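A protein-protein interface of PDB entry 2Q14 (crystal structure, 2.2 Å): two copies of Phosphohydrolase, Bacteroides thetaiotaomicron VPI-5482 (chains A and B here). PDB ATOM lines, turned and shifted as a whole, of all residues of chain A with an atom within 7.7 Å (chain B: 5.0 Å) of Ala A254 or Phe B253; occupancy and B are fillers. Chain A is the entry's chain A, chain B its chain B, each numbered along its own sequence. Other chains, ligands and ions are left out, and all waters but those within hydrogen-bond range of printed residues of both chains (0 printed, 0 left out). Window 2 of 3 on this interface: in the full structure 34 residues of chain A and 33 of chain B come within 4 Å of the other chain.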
ATOM      1  N   GLU A 251       5.977 -11.548 -38.593  1.00  0.00           N
ATOM      2  CA  GLU A 251       5.950 -11.728 -37.122  1.00  0.00           C
ATOM      3  C   GLU A 251       7.118 -12.593 -36.660  1.00  0.00           C
ATOM      4  O   GLU A 251       7.292 -13.733 -37.111  1.00  0.00           O
ATOM      5  CB  GLU A 251       4.636 -12.368 -36.639  1.00  0.00           C
ATOM      6  CG  GLU A 251       4.279 -12.044 -35.182  1.00  0.00           C
ATOM      7  N   LEU A 252       7.928 -12.028 -35.775  1.00  0.00           N
ATOM      8  CA  LEU A 252       9.074 -12.717 -35.209  1.00  0.00           C
ATOM      9  C   LEU A 252       8.905 -12.775 -33.720  1.00  0.00           C
ATOM     10  O   LEU A 252       8.525 -11.795 -33.115  1.00  0.00           O
ATOM     11  CB  LEU A 252      10.344 -11.941 -35.492  1.00  0.00           C
ATOM     12  CG  LEU A 252      10.748 -11.799 -36.937  1.00  0.00           C
ATOM     13  CD1 LEU A 252      11.875 -10.851 -36.998  1.00  0.00           C
ATOM     14  CD2 LEU A 252      11.145 -13.124 -37.461  1.00  0.00           C
ATOM     15  N   PHE A 253       9.194 -13.914 -33.122  1.00  0.00           N
ATOM     16  CA  PHE A 253       9.270 -13.974 -31.685  1.00  0.00           C
ATOM     17  C   PHE A 253      10.350 -13.029 -31.155  1.00  0.00           C
ATOM     18  O   PHE A 253      11.462 -13.018 -31.667  1.00  0.00           O
ATOM     19  CB  PHE A 253       9.573 -15.396 -31.220  1.00  0.00           C
ATOM     20  CG  PHE A 253       9.697 -15.525 -29.728  1.00  0.00           C
ATOM     21  CD1 PHE A 253      10.875 -15.189 -29.083  1.00  0.00           C
ATOM     22  CD2 PHE A 253       8.629 -15.955 -28.975  1.00  0.00           C
ATOM     23  CE1 PHE A 253      10.982 -15.306 -27.721  1.00  0.00           C
ATOM     24  CE2 PHE A 253       8.732 -16.073 -27.613  1.00  0.00           C
ATOM     25  CZ  PHE A 253       9.913 -15.756 -26.986  1.00  0.00           C
ATOM     26  N   ALA A 254      10.002 -12.257 -30.132  1.00  0.00           N
ATOM     27  CA  ALA A 254      10.932 -11.364 -29.454  1.00  0.00           C
ATOM     28  C   ALA A 254      10.383 -10.850 -28.125  1.00  0.00           C
ATOM     29  O   ALA A 254       9.201 -10.574 -27.993  1.00  0.00           O
ATOM     30  CB  ALA A 254      11.325 -10.180 -30.353  1.00  0.00           C
ATOM     31  N   SER A 255      11.264 -10.708 -27.140  1.00  0.00           N
ATOM     32  CA  SER A 255      10.949  -9.959 -25.924  1.00  0.00           C
ATOM     33  C   SER A 255      10.571  -8.551 -26.332  1.00  0.00           C
ATOM     34  O   SER A 255      10.996  -8.094 -27.361  1.00  0.00           O
ATOM     35  CB  SER A 255      12.155  -9.929 -24.948  1.00  0.00           C
ATOM     36  OG  SER A 255      13.299  -9.201 -25.473  1.00  0.00           O
ATOM     37  N   PRO A 256       9.743  -7.869 -25.534  1.00  0.00           N
ATOM     38  CA  PRO A 256       9.418  -6.487 -25.807  1.00  0.00           C
ATOM     39  C   PRO A 256      10.625  -5.591 -26.050  1.00  0.00           C
ATOM     40  O   PRO A 256      10.591  -4.778 -26.962  1.00  0.00           O
ATOM     41  CB  PRO A 256       8.675  -6.049 -24.550  1.00  0.00           C
ATOM     42  CG  PRO A 256       8.082  -7.244 -24.036  1.00  0.00           C
ATOM     43  CD  PRO A 256       9.000  -8.376 -24.370  1.00  0.00           C
ATOM     44  N   ALA A 257      11.674  -5.721 -25.240  1.00  0.00           N
ATOM     45  CA  ALA A 257      12.869  -4.898 -25.447  1.00  0.00           C
ATOM     46  C   ALA A 257      13.489  -5.141 -26.817  1.00  0.00           C
ATOM     47  O   ALA A 257      13.820  -4.188 -27.515  1.00  0.00           O
ATOM     48  CB  ALA A 257      13.893  -5.108 -24.336  1.00  0.00           C
ATOM     49  N   LEU A 258      13.612  -6.404 -27.226  1.00  0.00           N
ATOM     50  CA  LEU A 258      14.208  -6.716 -28.537  1.00  0.00           C
ATOM     51  C   LEU A 258      13.292  -6.317 -29.682  1.00  0.00           C
ATOM     52  O   LEU A 258      13.740  -5.743 -30.705  1.00  0.00           O
ATOM     53  CB  LEU A 258      14.561  -8.186 -28.634  1.00  0.00           C
ATOM     54  CG  LEU A 258      15.174  -8.703 -29.925  1.00  0.00           C
ATOM     55  CD1 LEU A 258      16.503  -8.011 -30.218  1.00  0.00           C
ATOM     56  CD2 LEU A 258      15.321 -10.210 -29.794  1.00  0.00           C
ATOM     57  N   HIS A 259      12.006  -6.604 -29.506  1.00  0.00           N
ATOM     58  CA  HIS A 259      10.963  -6.166 -30.438  1.00  0.00           C
ATOM     59  C   HIS A 259      11.072  -4.671 -30.788  1.00  0.00           C
ATOM     60  O   HIS A 259      11.034  -4.271 -31.948  1.00  0.00           O
ATOM     61  CB  HIS A 259       9.613  -6.469 -29.811  1.00  0.00           C
ATOM     62  CG  HIS A 259       8.476  -6.412 -30.774  1.00  0.00           C
ATOM     63  ND1 HIS A 259       7.838  -5.232 -31.102  1.00  0.00           N
ATOM     64  CD2 HIS A 259       7.861  -7.391 -31.478  1.00  0.00           C
ATOM     65  CE1 HIS A 259       6.888  -5.489 -31.978  1.00  0.00           C
ATOM     66  NE2 HIS A 259       6.881  -6.788 -32.224  1.00  0.00           N
ATOM     67  N   PHE A 260      11.243  -3.841 -29.781  1.00  0.00           N
ATOM     68  CA  PHE A 260      11.452  -2.413 -30.017  1.00  0.00           C
ATOM     69  C   PHE A 260      12.491  -2.090 -31.119  1.00  0.00           C
ATOM     70  O   PHE A 260      12.276  -1.217 -31.948  1.00  0.00           O
ATOM     71  CB  PHE A 260      11.831  -1.745 -28.699  1.00  0.00           C
ATOM     72  CG  PHE A 260      11.936  -0.265 -28.794  1.00  0.00           C
ATOM     73  CD1 PHE A 260      10.803   0.512 -28.729  1.00  0.00           C
ATOM     74  CD2 PHE A 260      13.159   0.338 -29.010  1.00  0.00           C
ATOM     75  CE1 PHE A 260      10.881   1.858 -28.870  1.00  0.00           C
ATOM     76  CE2 PHE A 260      13.248   1.695 -29.158  1.00  0.00           C
ATOM     77  CZ  PHE A 260      12.117   2.461 -29.074  1.00  0.00           C
ATOM     78  N   LEU A 262      13.769  -4.254 -33.430  1.00  0.00           N
ATOM     79  CA  LEU A 262      13.483  -4.983 -34.653  1.00  0.00           C
ATOM     80  C   LEU A 262      12.387  -4.291 -35.492  1.00  0.00           C
ATOM     81  O   LEU A 262      12.445  -4.305 -36.711  1.00  0.00           O
ATOM     82  CB  LEU A 262      13.078  -6.421 -34.334  1.00  0.00           C
ATOM     83  CG  LEU A 262      14.182  -7.391 -33.884  1.00  0.00           C
ATOM     84  CD1 LEU A 262      13.607  -8.774 -33.627  1.00  0.00           C
ATOM     85  CD2 LEU A 262      15.330  -7.487 -34.920  1.00  0.00           C
ATOM     86  N   TYR A 263      11.412  -3.697 -34.823  1.00  0.00           N
ATOM     87  CA  TYR A 263      10.211  -3.176 -35.446  1.00  0.00           C
ATOM     88  C   TYR A 263      10.199  -1.655 -35.536  1.00  0.00           C
ATOM     89  O   TYR A 263       9.219  -1.085 -35.974  1.00  0.00           O
ATOM     90  CB  TYR A 263       8.961  -3.701 -34.698  1.00  0.00           C
ATOM     91  CG  TYR A 263       8.688  -5.143 -35.033  1.00  0.00           C
ATOM     92  CD1 TYR A 263       9.302  -6.166 -34.325  1.00  0.00           C
ATOM     93  CD2 TYR A 263       7.883  -5.494 -36.110  1.00  0.00           C
ATOM     94  CE1 TYR A 263       9.102  -7.510 -34.654  1.00  0.00           C
ATOM     95  CE2 TYR A 263       7.671  -6.850 -36.454  1.00  0.00           C
ATOM     96  CZ  TYR A 263       8.279  -7.857 -35.710  1.00  0.00           C
ATOM     97  OH  TYR A 263       8.095  -9.206 -36.015  1.00  0.00           O
ATOM     98  N   ASP A 288      17.892 -12.239 -24.219  1.00  0.00           N
ATOM     99  CA  ASP A 288      17.034 -11.742 -25.279  1.00  0.00           C
ATOM    100  C   ASP A 288      17.526 -12.174 -26.645  1.00  0.00           C
ATOM    101  O   ASP A 288      16.738 -12.557 -27.474  1.00  0.00           O
ATOM    102  CB  ASP A 288      16.927 -10.219 -25.235  1.00  0.00           C
ATOM    103  CG  ASP A 288      16.357  -9.710 -23.917  1.00  0.00           C
ATOM    104  OD1 ASP A 288      15.132  -9.846 -23.710  1.00  0.00           O
ATOM    105  OD2 ASP A 288      17.140  -9.172 -23.088  1.00  0.00           O
ATOM    106  N   THR A 291      17.284 -16.277 -26.864  1.00  0.00           N
ATOM    107  CA  THR A 291      15.927 -16.751 -26.934  1.00  0.00           C
ATOM    108  C   THR A 291      15.380 -16.525 -28.338  1.00  0.00           C
ATOM    109  O   THR A 291      14.796 -17.434 -28.916  1.00  0.00           O
ATOM    110  CB  THR A 291      15.079 -16.152 -25.845  1.00  0.00           C
ATOM    111  OG1 THR A 291      15.654 -16.539 -24.608  1.00  0.00           O
ATOM    112  CG2 THR A 291      13.661 -16.713 -25.916  1.00  0.00           C
ATOM    113  N   ALA A 292      15.640 -15.356 -28.902  1.00  0.00           N
ATOM    114  CA  ALA A 292      15.234 -15.074 -30.266  1.00  0.00           C
ATOM    115  C   ALA A 292      15.815 -16.124 -31.219  1.00  0.00           C
ATOM    116  O   ALA A 292      15.097 -16.769 -31.936  1.00  0.00           O
ATOM    117  CB  ALA A 292      15.637 -13.660 -30.675  1.00  0.00           C
ATOM    118  N   VAL A 295      14.079 -19.610 -30.916  1.00  0.00           N
ATOM    119  CA  VAL A 295      12.734 -19.670 -31.487  1.00  0.00           C
ATOM    120  C   VAL A 295      12.765 -19.467 -33.009  1.00  0.00           C
ATOM    121  O   VAL A 295      12.059 -20.135 -33.754  1.00  0.00           O
ATOM    122  CB  VAL A 295      11.771 -18.660 -30.793  1.00  0.00           C
ATOM    123  CG1 VAL A 295      10.342 -18.848 -31.296  1.00  0.00           C
ATOM    124  CG2 VAL A 295      11.836 -18.853 -29.294  1.00  0.00           C
ATOM    125  N   TRP A 296      13.625 -18.582 -33.472  1.00  0.00           N
ATOM    126  CA  TRP A 296      13.735 -18.319 -34.897  1.00  0.00           C
ATOM    127  C   TRP A 296      14.317 -19.494 -35.638  1.00  0.00           C
ATOM    128  O   TRP A 296      14.191 -19.555 -36.852  1.00  0.00           O
ATOM    129  CB  TRP A 296      14.586 -17.101 -35.189  1.00  0.00           C
ATOM    130  CG  TRP A 296      14.063 -15.840 -34.654  1.00  0.00           C
ATOM    131  CD1 TRP A 296      12.808 -15.585 -34.174  1.00  0.00           C
ATOM    132  CD2 TRP A 296      14.796 -14.643 -34.519  1.00  0.00           C
ATOM    133  NE1 TRP A 296      12.720 -14.287 -33.779  1.00  0.00           N
ATOM    134  CE2 TRP A 296      13.945 -13.694 -33.957  1.00  0.00           C
ATOM    135  CE3 TRP A 296      16.107 -14.277 -34.833  1.00  0.00           C
ATOM    136  CZ2 TRP A 296      14.356 -12.401 -33.701  1.00  0.00           C
ATOM    137  CZ3 TRP A 296      16.516 -13.006 -34.566  1.00  0.00           C
ATOM    138  CH2 TRP A 296      15.644 -12.077 -34.008  1.00  0.00           C
ATOM    139  N   GLU B 251      -2.312 -14.434 -19.495  1.00  0.00           N
ATOM    140  CA  GLU B 251      -1.243 -14.417 -20.502  1.00  0.00           C
ATOM    141  C   GLU B 251       0.100 -14.129 -19.853  1.00  0.00           C
ATOM    142  O   GLU B 251       0.254 -13.143 -19.134  1.00  0.00           O
ATOM    143  CB  GLU B 251      -1.483 -13.332 -21.542  1.00  0.00           C
ATOM    144  CG  GLU B 251      -2.645 -13.563 -22.464  1.00  0.00           C
ATOM    145  CD  GLU B 251      -2.713 -12.481 -23.535  1.00  0.00           C
ATOM    146  OE1 GLU B 251      -2.024 -12.632 -24.562  1.00  0.00           O
ATOM    147  OE2 GLU B 251      -3.423 -11.471 -23.339  1.00  0.00           O
ATOM    148  N   LEU B 252       1.062 -14.984 -20.146  1.00  0.00           N
ATOM    149  CA  LEU B 252       2.409 -14.837 -19.667  1.00  0.00           C
ATOM    150  C   LEU B 252       3.356 -14.959 -20.842  1.00  0.00           C
ATOM    151  O   LEU B 252       3.219 -15.899 -21.614  1.00  0.00           O
ATOM    152  CB  LEU B 252       2.715 -15.955 -18.672  1.00  0.00           C
ATOM    153  CG  LEU B 252       1.985 -15.997 -17.336  1.00  0.00           C
ATOM    154  CD1 LEU B 252       2.380 -17.236 -16.573  1.00  0.00           C
ATOM    155  CD2 LEU B 252       2.302 -14.809 -16.531  1.00  0.00           C
ATOM    156  N   PHE B 253       4.309 -14.030 -20.972  1.00  0.00           N
ATOM    157  CA  PHE B 253       5.377 -14.170 -21.940  1.00  0.00           C
ATOM    158  C   PHE B 253       6.128 -15.492 -21.739  1.00  0.00           C
ATOM    159  O   PHE B 253       6.497 -15.847 -20.613  1.00  0.00           O
ATOM    160  CB  PHE B 253       6.377 -13.031 -21.832  1.00  0.00           C
ATOM    161  CG  PHE B 253       7.378 -13.041 -22.927  1.00  0.00           C
ATOM    162  CD1 PHE B 253       8.561 -13.744 -22.786  1.00  0.00           C
ATOM    163  CD2 PHE B 253       7.093 -12.436 -24.141  1.00  0.00           C
ATOM    164  CE1 PHE B 253       9.470 -13.783 -23.813  1.00  0.00           C
ATOM    165  CE2 PHE B 253       7.991 -12.481 -25.170  1.00  0.00           C
ATOM    166  CZ  PHE B 253       9.195 -13.157 -24.997  1.00  0.00           C
ATOM    167  N   ALA B 254       6.349 -16.221 -22.825  1.00  0.00           N
ATOM    168  CA  ALA B 254       7.134 -17.438 -22.766  1.00  0.00           C
ATOM    169  C   ALA B 254       7.463 -17.883 -24.156  1.00  0.00           C
ATOM    170  O   ALA B 254       6.686 -17.690 -25.079  1.00  0.00           O
ATOM    171  CB  ALA B 254       6.390 -18.542 -22.022  1.00  0.00           C
ATOM    172  N   SER B 255       8.651 -18.456 -24.302  1.00  0.00           N
ATOM    173  CA  SER B 255       9.047 -19.172 -25.509  1.00  0.00           C
ATOM    174  C   SER B 255       8.095 -20.355 -25.673  1.00  0.00           C
ATOM    175  O   SER B 255       7.537 -20.824 -24.691  1.00  0.00           O
ATOM    176  CB  SER B 255      10.485 -19.670 -25.373  1.00  0.00           C
ATOM    177  OG  SER B 255      10.593 -20.685 -24.378  1.00  0.00           O
ATOM    178  N   THR B 291      14.654 -15.175 -19.807  1.00  0.00           N
ATOM    179  CA  THR B 291      13.816 -14.267 -20.610  1.00  0.00           C
ATOM    180  C   THR B 291      12.426 -14.142 -19.952  1.00  0.00           C
ATOM    181  O   THR B 291      11.906 -13.058 -19.834  1.00  0.00           O
ATOM    182  CB  THR B 291      13.745 -14.635 -22.117  1.00  0.00           C
ATOM    183  OG1 THR B 291      14.992 -15.168 -22.520  1.00  0.00           O
ATOM    184  CG2 THR B 291      13.551 -13.404 -22.987  1.00  0.00           C
ATOM    185  N   ALA B 292      11.864 -15.243 -19.479  1.00  0.00           N
ATOM    186  CA  ALA B 292      10.591 -15.201 -18.770  1.00  0.00           C
ATOM    187  C   ALA B 292      10.638 -14.295 -17.531  1.00  0.00           C
ATOM    188  O   ALA B 292       9.816 -13.412 -17.382  1.00  0.00           O
ATOM    189  CB  ALA B 292      10.161 -16.591 -18.396  1.00  0.00           C
ATOM    190  N   VAL B 295      10.820 -10.539 -18.525  1.00  0.00           N
ATOM    191  CA  VAL B 295       9.566  -9.971 -18.985  1.00  0.00           C
ATOM    192  C   VAL B 295       8.524  -9.968 -17.839  1.00  0.00           C
ATOM    193  O   VAL B 295       7.804  -9.006 -17.656  1.00  0.00           O
ATOM    194  CB  VAL B 295       9.050 -10.661 -20.251  1.00  0.00           C
ATOM    195  CG1 VAL B 295       7.761 -10.009 -20.741  1.00  0.00           C
ATOM    196  CG2 VAL B 295      10.084 -10.564 -21.344  1.00  0.00           C
ATOM    197  N   TRP B 296       8.509 -11.020 -17.027  1.00  0.00           N
ATOM    198  CA  TRP B 296       7.527 -11.127 -15.958  1.00  0.00           C
ATOM    199  C   TRP B 296       7.754 -10.099 -14.885  1.00  0.00           C
ATOM    200  O   TRP B 296       6.853  -9.817 -14.092  1.00  0.00           O
ATOM    201  CB  TRP B 296       7.529 -12.519 -15.315  1.00  0.00           C
ATOM    202  CG  TRP B 296       7.104 -13.650 -16.235  1.00  0.00           C
ATOM    203  CD1 TRP B 296       6.519 -13.541 -17.467  1.00  0.00           C
ATOM    204  CD2 TRP B 296       7.264 -15.038 -15.994  1.00  0.00           C
ATOM    205  NE1 TRP B 296       6.325 -14.770 -18.008  1.00  0.00           N
ATOM    206  CE2 TRP B 296       6.762 -15.718 -17.126  1.00  0.00           C
ATOM    207  CE3 TRP B 296       7.824 -15.787 -14.943  1.00  0.00           C
ATOM    208  CZ2 TRP B 296       6.767 -17.114 -17.231  1.00  0.00           C
ATOM    209  CZ3 TRP B 296       7.830 -17.182 -15.050  1.00  0.00           C
ATOM    210  CH2 TRP B 296       7.291 -17.831 -16.186  1.00  0.00           C
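The side-chain hydroxyl (OG1) of Thr A291 is in hydrogen-bond range of the side-chain hydroxyl (OG1) of Thr B291, at 2.6 Å.
Among the printed residues, pairs that only touch across the chains: Phe A253 with Phe B253 (3.4 Å), Phe A253 with Ala B254 (3.6 Å), Phe A253 with Ser B255 (3.8 Å), Ala A254 with Phe B253 (3.6 Å), Ser A255 with Phe B253 (3.8 Å), Pro A256 with Val B295 (3.9 Å) and Asp A288 with Thr B291 (3.96 Å).
Ala A254 touches just one residue of chain B: Phe B253.
Of chain A, only Phe A253 (3.4 Å), Ala A254 (3.6 Å) and Ser A255 (3.8 Å) come within 4 Å of Phe B253.
Of the printed residues of chain A, Ala B254 touches Phe A253.
Of the printed residues of chain B, Thr A291 touches Thr B291.
Tyr A263 touches none of the printed residues of chain B.
The nearest printed residue of chain B that does not touch Ser A255 is Val B295 (4.2 Å).
Of the 9 printed residues of chain B, 5 touch a printed residue of chain A.
Printed residues of chain B that touch a printed residue of chain A: Phe B253, Ala B254, Ser B255, Thr B291 and Val B295.
Of the 17 printed residues of chain A, 6 touch a printed residue of chain B.
Printed residues of chain A that touch a printed residue of chain B: Phe A253, Ala A254, Ser A255, Pro A256, Asp A288 and Thr A291.
Among the printed residues, no Asp or Glu carboxylate lies within 4 Å of a Lys or Arg side-chain nitrogen of the other chain.
The indole nitrogen of Trp B296 sits at hydrogen-bond distance from the backbone carbonyl oxygen of Phe B253, 2.8 Å away.
The indole nitrogen (NE1) of Trp A296 is in hydrogen-bond range of the backbone carbonyl oxygen (O) of Phe A253 (2.8 Å).
The backbone NH (N) of Leu A258 sits at hydrogen-bond distance from the side-chain hydroxyl (OG) of Ser A255, 3.3 Å away.
OG of Ser A255 lies within hydrogen-bond range of OD1 of Asp A288, 2.6 Å away.
Phe B253 touches its own counterpart, Phe A253.
Phe A253 touches Ala B254, and with the chains exchanged Ala A254 touches Phe B253.
Phe A253 touches Ser B255, and with the chains exchanged Ser A255 touches Phe B253.
Thr B291 touches its own counterpart, Thr A291.
Positions printed for both chains: 251, 252, 253, 254, 255, 291, 292, 295 and 296.
Of the 8 pairs that touch across the chains among the printed residues, 6 have their exchanged pair printed and touching as well.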
